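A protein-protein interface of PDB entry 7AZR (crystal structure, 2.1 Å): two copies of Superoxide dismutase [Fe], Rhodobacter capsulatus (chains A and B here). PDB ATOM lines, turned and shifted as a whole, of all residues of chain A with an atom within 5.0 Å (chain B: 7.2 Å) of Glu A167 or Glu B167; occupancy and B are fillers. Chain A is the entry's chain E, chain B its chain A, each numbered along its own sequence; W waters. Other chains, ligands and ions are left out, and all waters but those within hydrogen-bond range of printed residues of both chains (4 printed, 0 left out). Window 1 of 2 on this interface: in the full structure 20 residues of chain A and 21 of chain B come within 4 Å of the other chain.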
ATOM      1  N   HIS A  31     -36.232   2.000 -15.995  1.00  0.00           N
ATOM      2  CA  HIS A  31     -35.608   1.423 -17.188  1.00  0.00           C
ATOM      3  C   HIS A  31     -36.507   0.384 -17.868  1.00  0.00           C
ATOM      4  O   HIS A  31     -36.773   0.481 -19.059  1.00  0.00           O
ATOM      5  CB  HIS A  31     -34.234   0.805 -16.889  1.00  0.00           C
ATOM      6  CG  HIS A  31     -33.173   1.808 -16.571  1.00  0.00           C
ATOM      7  ND1 HIS A  31     -32.439   2.443 -17.547  1.00  0.00           N
ATOM      8  CD2 HIS A  31     -32.708   2.276 -15.384  1.00  0.00           C
ATOM      9  CE1 HIS A  31     -31.578   3.270 -16.978  1.00  0.00           C
ATOM     10  NE2 HIS A  31     -31.713   3.182 -15.665  1.00  0.00           N
ATOM     11  N   VAL A 165     -25.321  -6.670 -17.714  1.00  0.00           N
ATOM     12  CA  VAL A 165     -24.090  -5.913 -17.494  1.00  0.00           C
ATOM     13  C   VAL A 165     -24.123  -4.519 -18.106  1.00  0.00           C
ATOM     14  O   VAL A 165     -23.103  -3.850 -18.177  1.00  0.00           O
ATOM     15  CB  VAL A 165     -22.815  -6.690 -17.865  1.00  0.00           C
ATOM     16  CG1 VAL A 165     -22.677  -7.904 -16.960  1.00  0.00           C
ATOM     17  CG2 VAL A 165     -22.814  -7.093 -19.331  1.00  0.00           C
ATOM     18  N   TRP A 166     -25.309  -4.046 -18.483  1.00  0.00           N
ATOM     19  CA  TRP A 166     -25.485  -2.602 -18.636  1.00  0.00           C
ATOM     20  C   TRP A 166     -25.108  -1.964 -17.298  1.00  0.00           C
ATOM     21  O   TRP A 166     -25.425  -2.491 -16.231  1.00  0.00           O
ATOM     22  CB  TRP A 166     -26.915  -2.227 -18.959  1.00  0.00           C
ATOM     23  CG  TRP A 166     -27.414  -2.542 -20.328  1.00  0.00           C
ATOM     24  CD1 TRP A 166     -27.479  -3.765 -20.924  1.00  0.00           C
ATOM     25  CD2 TRP A 166     -28.008  -1.612 -21.251  1.00  0.00           C
ATOM     26  NE1 TRP A 166     -28.082  -3.666 -22.159  1.00  0.00           N
ATOM     27  CE2 TRP A 166     -28.417  -2.352 -22.384  1.00  0.00           C
ATOM     28  CE3 TRP A 166     -28.245  -0.234 -21.222  1.00  0.00           C
ATOM     29  CZ2 TRP A 166     -29.028  -1.755 -23.484  1.00  0.00           C
ATOM     30  CZ3 TRP A 166     -28.864   0.353 -22.297  1.00  0.00           C
ATOM     31  CH2 TRP A 166     -29.252  -0.409 -23.423  1.00  0.00           C
ATOM     32  N   GLU A 167     -24.445  -0.804 -17.357  1.00  0.00           N
ATOM     33  CA  GLU A 167     -23.940  -0.150 -16.164  1.00  0.00           C
ATOM     34  C   GLU A 167     -25.044   0.234 -15.173  1.00  0.00           C
ATOM     35  O   GLU A 167     -24.815   0.191 -13.959  1.00  0.00           O
ATOM     36  CB  GLU A 167     -23.061   1.042 -16.546  1.00  0.00           C
ATOM     37  CG  GLU A 167     -21.684   0.609 -17.079  1.00  0.00           C
ATOM     38  CD  GLU A 167     -20.845   1.763 -17.579  1.00  0.00           C
ATOM     39  OE1 GLU A 167     -21.410   2.685 -18.224  1.00  0.00           O
ATOM     40  OE2 GLU A 167     -19.612   1.760 -17.315  1.00  0.00           O
ATOM     41  N   HIS A 168     -26.254   0.537 -15.674  1.00  0.00           N
ATOM     42  CA  HIS A 168     -27.363   0.898 -14.779  1.00  0.00           C
ATOM     43  C   HIS A 168     -27.727  -0.233 -13.808  1.00  0.00           C
ATOM     44  O   HIS A 168     -28.257   0.018 -12.735  1.00  0.00           O
ATOM     45  CB  HIS A 168     -28.606   1.424 -15.520  1.00  0.00           C
ATOM     46  CG  HIS A 168     -29.285   0.429 -16.411  1.00  0.00           C
ATOM     47  ND1 HIS A 168     -29.431   0.631 -17.761  1.00  0.00           N
ATOM     48  CD2 HIS A 168     -29.897  -0.748 -16.138  1.00  0.00           C
ATOM     49  CE1 HIS A 168     -30.082  -0.390 -18.291  1.00  0.00           C
ATOM     50  NE2 HIS A 168     -30.366  -1.249 -17.327  1.00  0.00           N
ATOM     51  N   SER A 169     -27.427  -1.477 -14.195  1.00  0.00           N
ATOM     52  CA  SER A 169     -27.749  -2.640 -13.371  1.00  0.00           C
ATOM     53  C   SER A 169     -26.928  -2.714 -12.087  1.00  0.00           C
ATOM     54  O   SER A 169     -27.376  -3.328 -11.123  1.00  0.00           O
ATOM     55  CB  SER A 169     -27.580  -3.931 -14.174  1.00  0.00           C
ATOM     56  OG  SER A 169     -28.160  -5.012 -13.466  1.00  0.00           O
ATOM     57  N   TYR A 170     -25.745  -2.084 -12.085  1.00  0.00           N
ATOM     58  CA  TYR A 170     -24.823  -2.170 -10.963  1.00  0.00           C
ATOM     59  C   TYR A 170     -24.182  -0.888 -10.475  1.00  0.00           C
ATOM     60  O   TYR A 170     -23.620  -0.883  -9.395  1.00  0.00           O
ATOM     61  CB  TYR A 170     -23.704  -3.188 -11.258  1.00  0.00           C
ATOM     62  CG  TYR A 170     -22.796  -2.871 -12.451  1.00  0.00           C
ATOM     63  CD1 TYR A 170     -21.657  -2.085 -12.317  1.00  0.00           C
ATOM     64  CD2 TYR A 170     -23.063  -3.404 -13.707  1.00  0.00           C
ATOM     65  CE1 TYR A 170     -20.816  -1.830 -13.405  1.00  0.00           C
ATOM     66  CE2 TYR A 170     -22.230  -3.169 -14.796  1.00  0.00           C
ATOM     67  CZ  TYR A 170     -21.113  -2.383 -14.643  1.00  0.00           C
ATOM     68  OH  TYR A 170     -20.311  -2.143 -15.736  1.00  0.00           O
ATOM     69  N   TYR A 171     -24.256   0.192 -11.259  1.00  0.00           N
ATOM     70  CA  TYR A 171     -23.447   1.370 -10.974  1.00  0.00           C
ATOM     71  C   TYR A 171     -23.745   2.023  -9.608  1.00  0.00           C
ATOM     72  O   TYR A 171     -22.840   2.530  -8.948  1.00  0.00           O
ATOM     73  CB  TYR A 171     -23.511   2.400 -12.109  1.00  0.00           C
ATOM     74  CG  TYR A 171     -22.187   3.097 -12.300  1.00  0.00           C
ATOM     75  CD1 TYR A 171     -21.127   2.443 -12.920  1.00  0.00           C
ATOM     76  CD2 TYR A 171     -21.970   4.386 -11.802  1.00  0.00           C
ATOM     77  CE1 TYR A 171     -19.892   3.051 -13.058  1.00  0.00           C
ATOM     78  CE2 TYR A 171     -20.740   5.021 -11.959  1.00  0.00           C
ATOM     79  CZ  TYR A 171     -19.701   4.356 -12.581  1.00  0.00           C
ATOM     80  OH  TYR A 171     -18.493   4.993 -12.724  1.00  0.00           O
ATOM     81  N   ARG A 178     -17.567  -3.946 -12.069  1.00  0.00           N
ATOM     82  CA  ARG A 178     -18.393  -4.958 -12.715  1.00  0.00           C
ATOM     83  C   ARG A 178     -17.990  -6.371 -12.290  1.00  0.00           C
ATOM     84  O   ARG A 178     -18.865  -7.202 -12.079  1.00  0.00           O
ATOM     85  CB  ARG A 178     -18.385  -4.832 -14.240  1.00  0.00           C
ATOM     86  CG  ARG A 178     -19.427  -5.734 -14.886  1.00  0.00           C
ATOM     87  CD  ARG A 178     -19.254  -5.882 -16.391  1.00  0.00           C
ATOM     88  NE  ARG A 178     -19.584  -4.652 -17.105  1.00  0.00           N
ATOM     89  CZ  ARG A 178     -19.633  -4.548 -18.421  1.00  0.00           C
ATOM     90  NH1 ARG A 178     -19.310  -5.578 -19.171  1.00  0.00           N
ATOM     91  NH2 ARG A 178     -19.955  -3.395 -18.985  1.00  0.00           N
ATOM     92  N   HIS B  31     -12.100   4.841 -14.833  1.00  0.00           N
ATOM     93  CA  HIS B  31     -12.484   4.359 -16.166  1.00  0.00           C
ATOM     94  C   HIS B  31     -11.431   4.693 -17.227  1.00  0.00           C
ATOM     95  O   HIS B  31     -10.970   3.821 -17.941  1.00  0.00           O
ATOM     96  CB  HIS B  31     -13.854   4.873 -16.594  1.00  0.00           C
ATOM     97  CG  HIS B  31     -15.001   4.286 -15.834  1.00  0.00           C
ATOM     98  ND1 HIS B  31     -15.613   3.111 -16.205  1.00  0.00           N
ATOM     99  CD2 HIS B  31     -15.684   4.739 -14.756  1.00  0.00           C
ATOM    100  CE1 HIS B  31     -16.605   2.850 -15.372  1.00  0.00           C
ATOM    101  NE2 HIS B  31     -16.678   3.831 -14.489  1.00  0.00           N
ATOM    102  N   TYR B  35      -8.670   2.221 -19.505  1.00  0.00           N
ATOM    103  CA  TYR B  35      -8.443   2.187 -20.956  1.00  0.00           C
ATOM    104  C   TYR B  35      -6.955   2.353 -21.295  1.00  0.00           C
ATOM    105  O   TYR B  35      -6.432   1.679 -22.187  1.00  0.00           O
ATOM    106  CB  TYR B  35      -9.279   3.233 -21.680  1.00  0.00           C
ATOM    107  CG  TYR B  35     -10.770   3.082 -21.489  1.00  0.00           C
ATOM    108  CD1 TYR B  35     -11.412   1.843 -21.675  1.00  0.00           C
ATOM    109  CD2 TYR B  35     -11.549   4.181 -21.108  1.00  0.00           C
ATOM    110  CE1 TYR B  35     -12.791   1.716 -21.514  1.00  0.00           C
ATOM    111  CE2 TYR B  35     -12.923   4.054 -20.932  1.00  0.00           C
ATOM    112  CZ  TYR B  35     -13.539   2.821 -21.137  1.00  0.00           C
ATOM    113  OH  TYR B  35     -14.887   2.704 -20.969  1.00  0.00           O
ATOM    114  N   GLY B 127     -27.621   1.559 -25.919  1.00  0.00           N
ATOM    115  CA  GLY B 127     -26.518   0.987 -25.180  1.00  0.00           C
ATOM    116  C   GLY B 127     -25.483   2.070 -24.879  1.00  0.00           C
ATOM    117  O   GLY B 127     -25.829   3.211 -24.595  1.00  0.00           O
ATOM    118  N   SER B 128     -24.204   1.692 -24.963  1.00  0.00           N
ATOM    119  CA  SER B 128     -23.087   2.571 -24.662  1.00  0.00           C
ATOM    120  C   SER B 128     -22.598   3.194 -25.952  1.00  0.00           C
ATOM    121  O   SER B 128     -22.622   2.556 -27.030  1.00  0.00           O
ATOM    122  CB  SER B 128     -21.942   1.759 -24.048  1.00  0.00           C
ATOM    123  OG  SER B 128     -22.344   1.067 -22.885  1.00  0.00           O
ATOM    124  N   GLY B 129     -22.115   4.429 -25.854  1.00  0.00           N
ATOM    125  CA  GLY B 129     -21.489   5.104 -26.994  1.00  0.00           C
ATOM    126  C   GLY B 129     -21.352   6.589 -26.805  1.00  0.00           C
ATOM    127  O   GLY B 129     -21.224   7.054 -25.680  1.00  0.00           O
ATOM    128  N   ASP B 164     -20.015  11.675 -24.112  1.00  0.00           N
ATOM    129  CA  ASP B 164     -20.039  10.288 -23.660  1.00  0.00           C
ATOM    130  C   ASP B 164     -21.440   9.956 -23.186  1.00  0.00           C
ATOM    131  O   ASP B 164     -21.964  10.632 -22.298  1.00  0.00           O
ATOM    132  CB  ASP B 164     -19.064  10.179 -22.507  1.00  0.00           C
ATOM    133  CG  ASP B 164     -18.749   8.768 -22.104  1.00  0.00           C
ATOM    134  OD1 ASP B 164     -19.301   7.808 -22.670  1.00  0.00           O
ATOM    135  OD2 ASP B 164     -17.906   8.658 -21.186  1.00  0.00           O
ATOM    136  N   VAL B 165     -22.083   8.976 -23.827  1.00  0.00           N
ATOM    137  CA  VAL B 165     -23.384   8.494 -23.329  1.00  0.00           C
ATOM    138  C   VAL B 165     -23.329   7.073 -22.768  1.00  0.00           C
ATOM    139  O   VAL B 165     -24.346   6.467 -22.518  1.00  0.00           O
ATOM    140  CB  VAL B 165     -24.528   8.694 -24.334  1.00  0.00           C
ATOM    141  CG1 VAL B 165     -24.749  10.187 -24.582  1.00  0.00           C
ATOM    142  CG2 VAL B 165     -24.286   7.955 -25.624  1.00  0.00           C
ATOM    143  N   TRP B 166     -22.122   6.557 -22.508  1.00  0.00           N
ATOM    144  CA  TRP B 166     -22.001   5.437 -21.592  1.00  0.00           C
ATOM    145  C   TRP B 166     -22.622   5.886 -20.264  1.00  0.00           C
ATOM    146  O   TRP B 166     -22.465   7.037 -19.849  1.00  0.00           O
ATOM    147  CB  TRP B 166     -20.561   5.062 -21.326  1.00  0.00           C
ATOM    148  CG  TRP B 166     -19.838   4.350 -22.421  1.00  0.00           C
ATOM    149  CD1 TRP B 166     -19.609   4.804 -23.678  1.00  0.00           C
ATOM    150  CD2 TRP B 166     -19.164   3.087 -22.315  1.00  0.00           C
ATOM    151  NE1 TRP B 166     -18.838   3.901 -24.373  1.00  0.00           N
ATOM    152  CE2 TRP B 166     -18.552   2.837 -23.558  1.00  0.00           C
ATOM    153  CE3 TRP B 166     -19.022   2.139 -21.281  1.00  0.00           C
ATOM    154  CZ2 TRP B 166     -17.828   1.679 -23.812  1.00  0.00           C
ATOM    155  CZ3 TRP B 166     -18.290   0.996 -21.527  1.00  0.00           C
ATOM    156  CH2 TRP B 166     -17.694   0.776 -22.779  1.00  0.00           C
ATOM    157  N   GLU B 167     -23.310   4.969 -19.588  1.00  0.00           N
ATOM    158  CA  GLU B 167     -24.056   5.319 -18.398  1.00  0.00           C
ATOM    159  C   GLU B 167     -23.159   5.830 -17.263  1.00  0.00           C
ATOM    160  O   GLU B 167     -23.590   6.695 -16.496  1.00  0.00           O
ATOM    161  CB  GLU B 167     -24.964   4.156 -17.960  1.00  0.00           C
ATOM    162  CG  GLU B 167     -26.149   3.973 -18.929  1.00  0.00           C
ATOM    163  CD  GLU B 167     -27.029   2.784 -18.623  1.00  0.00           C
ATOM    164  OE1 GLU B 167     -26.479   1.729 -18.288  1.00  0.00           O
ATOM    165  OE2 GLU B 167     -28.274   2.922 -18.684  1.00  0.00           O
ATOM    166  N   HIS B 168     -21.907   5.350 -17.188  1.00  0.00           N
ATOM    167  CA  HIS B 168     -20.983   5.801 -16.146  1.00  0.00           C
ATOM    168  C   HIS B 168     -20.719   7.311 -16.211  1.00  0.00           C
ATOM    169  O   HIS B 168     -20.390   7.911 -15.212  1.00  0.00           O
ATOM    170  CB  HIS B 168     -19.656   5.005 -16.093  1.00  0.00           C
ATOM    171  CG  HIS B 168     -18.788   5.126 -17.314  1.00  0.00           C
ATOM    172  ND1 HIS B 168     -18.433   4.036 -18.090  1.00  0.00           N
ATOM    173  CD2 HIS B 168     -18.186   6.204 -17.883  1.00  0.00           C
ATOM    174  CE1 HIS B 168     -17.649   4.440 -19.079  1.00  0.00           C
ATOM    175  NE2 HIS B 168     -17.497   5.753 -18.987  1.00  0.00           N
ATOM    176  N   SER B 169     -20.889   7.911 -17.394  1.00  0.00           N
ATOM    177  CA  SER B 169     -20.629   9.324 -17.590  1.00  0.00           C
ATOM    178  C   SER B 169     -21.631  10.220 -16.887  1.00  0.00           C
ATOM    179  O   SER B 169     -21.314  11.369 -16.603  1.00  0.00           O
ATOM    180  CB  SER B 169     -20.592   9.666 -19.081  1.00  0.00           C
ATOM    181  OG  SER B 169     -20.052  10.957 -19.262  1.00  0.00           O
ATOM    182  N   TYR B 170     -22.829   9.693 -16.604  1.00  0.00           N
ATOM    183  CA  TYR B 170     -23.910  10.477 -16.048  1.00  0.00           C
ATOM    184  C   TYR B 170     -24.701   9.853 -14.926  1.00  0.00           C
ATOM    185  O   TYR B 170     -25.431  10.569 -14.261  1.00  0.00           O
ATOM    186  CB  TYR B 170     -24.899  10.919 -17.151  1.00  0.00           C
ATOM    187  CG  TYR B 170     -25.619   9.796 -17.915  1.00  0.00           C
ATOM    188  CD1 TYR B 170     -26.811   9.241 -17.447  1.00  0.00           C
ATOM    189  CD2 TYR B 170     -25.114   9.312 -19.108  1.00  0.00           C
ATOM    190  CE1 TYR B 170     -27.470   8.239 -18.148  1.00  0.00           C
ATOM    191  CE2 TYR B 170     -25.773   8.309 -19.821  1.00  0.00           C
ATOM    192  CZ  TYR B 170     -26.956   7.777 -19.333  1.00  0.00           C
ATOM    193  OH  TYR B 170     -27.586   6.775 -20.061  1.00  0.00           O
ATOM    194  N   TYR B 171     -24.574   8.534 -14.713  1.00  0.00           N
ATOM    195  CA  TYR B 171     -25.485   7.831 -13.814  1.00  0.00           C
ATOM    196  C   TYR B 171     -25.448   8.349 -12.367  1.00  0.00           C
ATOM    197  O   TYR B 171     -26.478   8.381 -11.701  1.00  0.00           O
ATOM    198  CB  TYR B 171     -25.287   6.311 -13.857  1.00  0.00           C
ATOM    199  CG  TYR B 171     -26.616   5.586 -13.738  1.00  0.00           C
ATOM    200  CD1 TYR B 171     -27.503   5.547 -14.818  1.00  0.00           C
ATOM    201  CD2 TYR B 171     -27.011   5.001 -12.536  1.00  0.00           C
ATOM    202  CE1 TYR B 171     -28.740   4.939 -14.703  1.00  0.00           C
ATOM    203  CE2 TYR B 171     -28.242   4.360 -12.412  1.00  0.00           C
ATOM    204  CZ  TYR B 171     -29.106   4.326 -13.504  1.00  0.00           C
ATOM    205  OH  TYR B 171     -30.329   3.712 -13.401  1.00  0.00           O
ATOM    206  N   ILE B 172     -24.268   8.767 -11.893  1.00  0.00           N
ATOM    207  CA  ILE B 172     -24.135   9.327 -10.537  1.00  0.00           C
ATOM    208  C   ILE B 172     -24.963  10.598 -10.396  1.00  0.00           C
ATOM    209  O   ILE B 172     -25.635  10.789  -9.391  1.00  0.00           O
ATOM    210  CB  ILE B 172     -22.660   9.606 -10.163  1.00  0.00           C
ATOM    211  CG1 ILE B 172     -21.874   8.289 -10.074  1.00  0.00           C
ATOM    212  CG2 ILE B 172     -22.569  10.348  -8.826  1.00  0.00           C
ATOM    213  CD1 ILE B 172     -20.373   8.460 -10.205  1.00  0.00           C
ATOM    214  N   ASP B 173     -24.921  11.458 -11.419  1.00  0.00           N
ATOM    215  CA  ASP B 173     -25.527  12.778 -11.344  1.00  0.00           C
ATOM    216  C   ASP B 173     -26.955  12.847 -11.869  1.00  0.00           C
ATOM    217  O   ASP B 173     -27.725  13.652 -11.401  1.00  0.00           O
ATOM    218  CB  ASP B 173     -24.665  13.782 -12.101  1.00  0.00           C
ATOM    219  CG  ASP B 173     -23.239  13.795 -11.618  1.00  0.00           C
ATOM    220  OD1 ASP B 173     -23.017  13.715 -10.394  1.00  0.00           O
ATOM    221  OD2 ASP B 173     -22.332  13.862 -12.465  1.00  0.00           O
ATOM    222  N   ARG B 175     -28.774   9.679 -12.970  1.00  0.00           N
ATOM    223  CA  ARG B 175     -29.359   8.345 -13.033  1.00  0.00           C
ATOM    224  C   ARG B 175     -29.763   8.040 -14.486  1.00  0.00           C
ATOM    225  O   ARG B 175     -28.937   8.182 -15.384  1.00  0.00           O
ATOM    226  CB  ARG B 175     -30.513   8.232 -12.014  1.00  0.00           C
ATOM    227  CG  ARG B 175     -30.038   8.310 -10.569  1.00  0.00           C
ATOM    228  CD  ARG B 175     -29.456   6.971 -10.112  1.00  0.00           C
ATOM    229  NE  ARG B 175     -29.146   7.014  -8.690  1.00  0.00           N
ATOM    230  CZ  ARG B 175     -28.049   7.543  -8.155  1.00  0.00           C
ATOM    231  NH1 ARG B 175     -27.107   8.071  -8.921  1.00  0.00           N
ATOM    232  NH2 ARG B 175     -27.897   7.542  -6.828  1.00  0.00           N
ATOM    233  N   ASN B 176     -31.022   7.644 -14.704  1.00  0.00           N
ATOM    234  CA  ASN B 176     -31.547   7.273 -16.025  1.00  0.00           C
ATOM    235  C   ASN B 176     -31.810   8.430 -16.978  1.00  0.00           C
ATOM    236  O   ASN B 176     -32.159   8.205 -18.132  1.00  0.00           O
ATOM    237  CB  ASN B 176     -32.869   6.520 -15.861  1.00  0.00           C
ATOM    238  CG  ASN B 176     -33.930   7.371 -15.226  1.00  0.00           C
ATOM    239  OD1 ASN B 176     -33.774   7.809 -14.091  1.00  0.00           O
ATOM    240  ND2 ASN B 176     -35.000   7.632 -15.950  1.00  0.00           N
ATOM    241  N   ARG B 178     -30.771  10.423 -19.243  1.00  0.00           N
ATOM    242  CA  ARG B 178     -29.781  10.727 -20.252  1.00  0.00           C
ATOM    243  C   ARG B 178     -30.136  12.005 -21.014  1.00  0.00           C
ATOM    244  O   ARG B 178     -29.244  12.795 -21.303  1.00  0.00           O
ATOM    245  CB  ARG B 178     -29.559   9.557 -21.219  1.00  0.00           C
ATOM    246  CG  ARG B 178     -28.366   9.807 -22.133  1.00  0.00           C
ATOM    247  CD  ARG B 178     -28.308   8.857 -23.321  1.00  0.00           C
ATOM    248  NE  ARG B 178     -27.909   7.529 -22.903  1.00  0.00           N
ATOM    249  CZ  ARG B 178     -27.687   6.521 -23.739  1.00  0.00           C
ATOM    250  NH1 ARG B 178     -27.834   6.680 -25.046  1.00  0.00           N
ATOM    251  NH2 ARG B 178     -27.333   5.353 -23.263  1.00  0.00           N
HETATM  252  O   HOH W   1     -22.690   2.176 -20.494  1.00  0.00           O
HETATM  253  O   HOH W   2     -30.700   1.071 -12.136  1.00  0.00           O
HETATM  254  O   HOH W   3     -18.136   7.593 -13.638  1.00  0.00           O
HETATM  255  O   HOH W   4     -24.702   0.530 -19.985  1.00  0.00           O
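The side-chain hydroxyl (OH) of Tyr A171 is in hydrogen-bond range of a ring nitrogen (NE2) of His B31.
N of Glu B167 sits at hydrogen-bond distance from OE1 of Glu A167 (3.3 Å).
ND1 of His A168 is in hydrogen-bond range of OE2 of Glu B167, at 2.7 Å.
ND1 of His B168 lies within hydrogen-bond range of OE2 of Glu A167, at 2.7 Å.
A ring nitrogen (NE2) of His A31 is in hydrogen-bond range of the side-chain hydroxyl (OH) of Tyr B171 (2.7 Å).
Water W1 lies within hydrogen-bond range of OE1 of Glu A167 (2.7 Å), OG of Ser B128 (2.7 Å) and N of Glu B167 (3.0 Å).
Water W2 bridges the backbone carbonyl oxygen (O) of His A168 (2.7 Å) and the side-chain hydroxyl (OH) of Tyr B171 (3.0 Å).
Water W4 bridges the side-chain carboxylate (OE1) of Glu B167 and the backbone NH (N) of Glu A167.
Water W3 lies within hydrogen-bond range of O of His B168 (2.8 Å) and OH of Tyr A171 (2.8 Å).
Of the 18 printed residues of chain B, 8 touch a printed residue of chain A.
Hydrophobic or aromatic side chains of chain B within 4 Å of the printed part of chain A: His B31, Trp B166, His B168, Tyr B171 and Ile B172.
Printed residues of chain A that touch a printed residue of chain B: His A31, Trp A166, Glu A167, His A168 and Tyr A171.
Of chain B, only His B31, Trp B166, Glu B167 and His B168 come within 4 Å of Glu A167.
Glu B167 touches four residues of chain A.
Printed residues of chain A within 4 Å of His B168: Glu A167 (2.7 Å) and Tyr A171 (3.6 Å).
Printed residues of chain B within 4 Å of Tyr A171: His B31, His B168 and Ile B172.
The nearest residue of chain B that does not touch Glu A167 is Ser B128 (5.0 Å).
The nearest printed residue of chain A that does not touch Glu B167 is Ser A169 (5.3 Å).
The backbone carbonyl oxygen of Gly B127 lies within hydrogen-bond range of the guanidinium group of Arg B178, 2.9 Å away.
O of Gly B129 is in hydrogen-bond range of N of Trp B166 (3.3 Å).
The side-chain carboxylate of Asp B164 sits at hydrogen-bond distance from the backbone NH of Trp B166, 3.1 Å away.
The guanidinium group of Arg B175 sits at hydrogen-bond distance from the backbone carbonyl oxygen of Tyr B171, 2.9 Å away.
NH1 of Arg B175 lies within hydrogen-bond range of O of Ile B172 (3.1 Å).
Glu B167 touches His A31.
Asn B176 touches His A31 (CB to NE2, 3.5 Å).
CH2 of Trp A166 touches CA of Gly B127, at 3.5 Å.
CE3 of Trp A166 touches OE1 of Glu B167 (3.9 Å).
Glu A167 touches His B31.
OE1 of Glu A167 touches CE3 of Trp B166 (3.9 Å).
CB of His A168 touches OH of Tyr B171, at 3.6 Å.
OH of Tyr A171 touches CB of His B168, 3.6 Å away.
CE2 of Tyr A171 touches CD1 of Ile B172 (3.9 Å).
His A31 touches Glu B167, and with the chains exchanged Glu A167 touches His B31.
His A31 touches Tyr B171, and with the chains exchanged Tyr A171 touches His B31.
Glu A167 touches its own counterpart, Glu B167.
Glu A167 touches His B168, and with the chains exchanged His A168 touches Glu B167.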
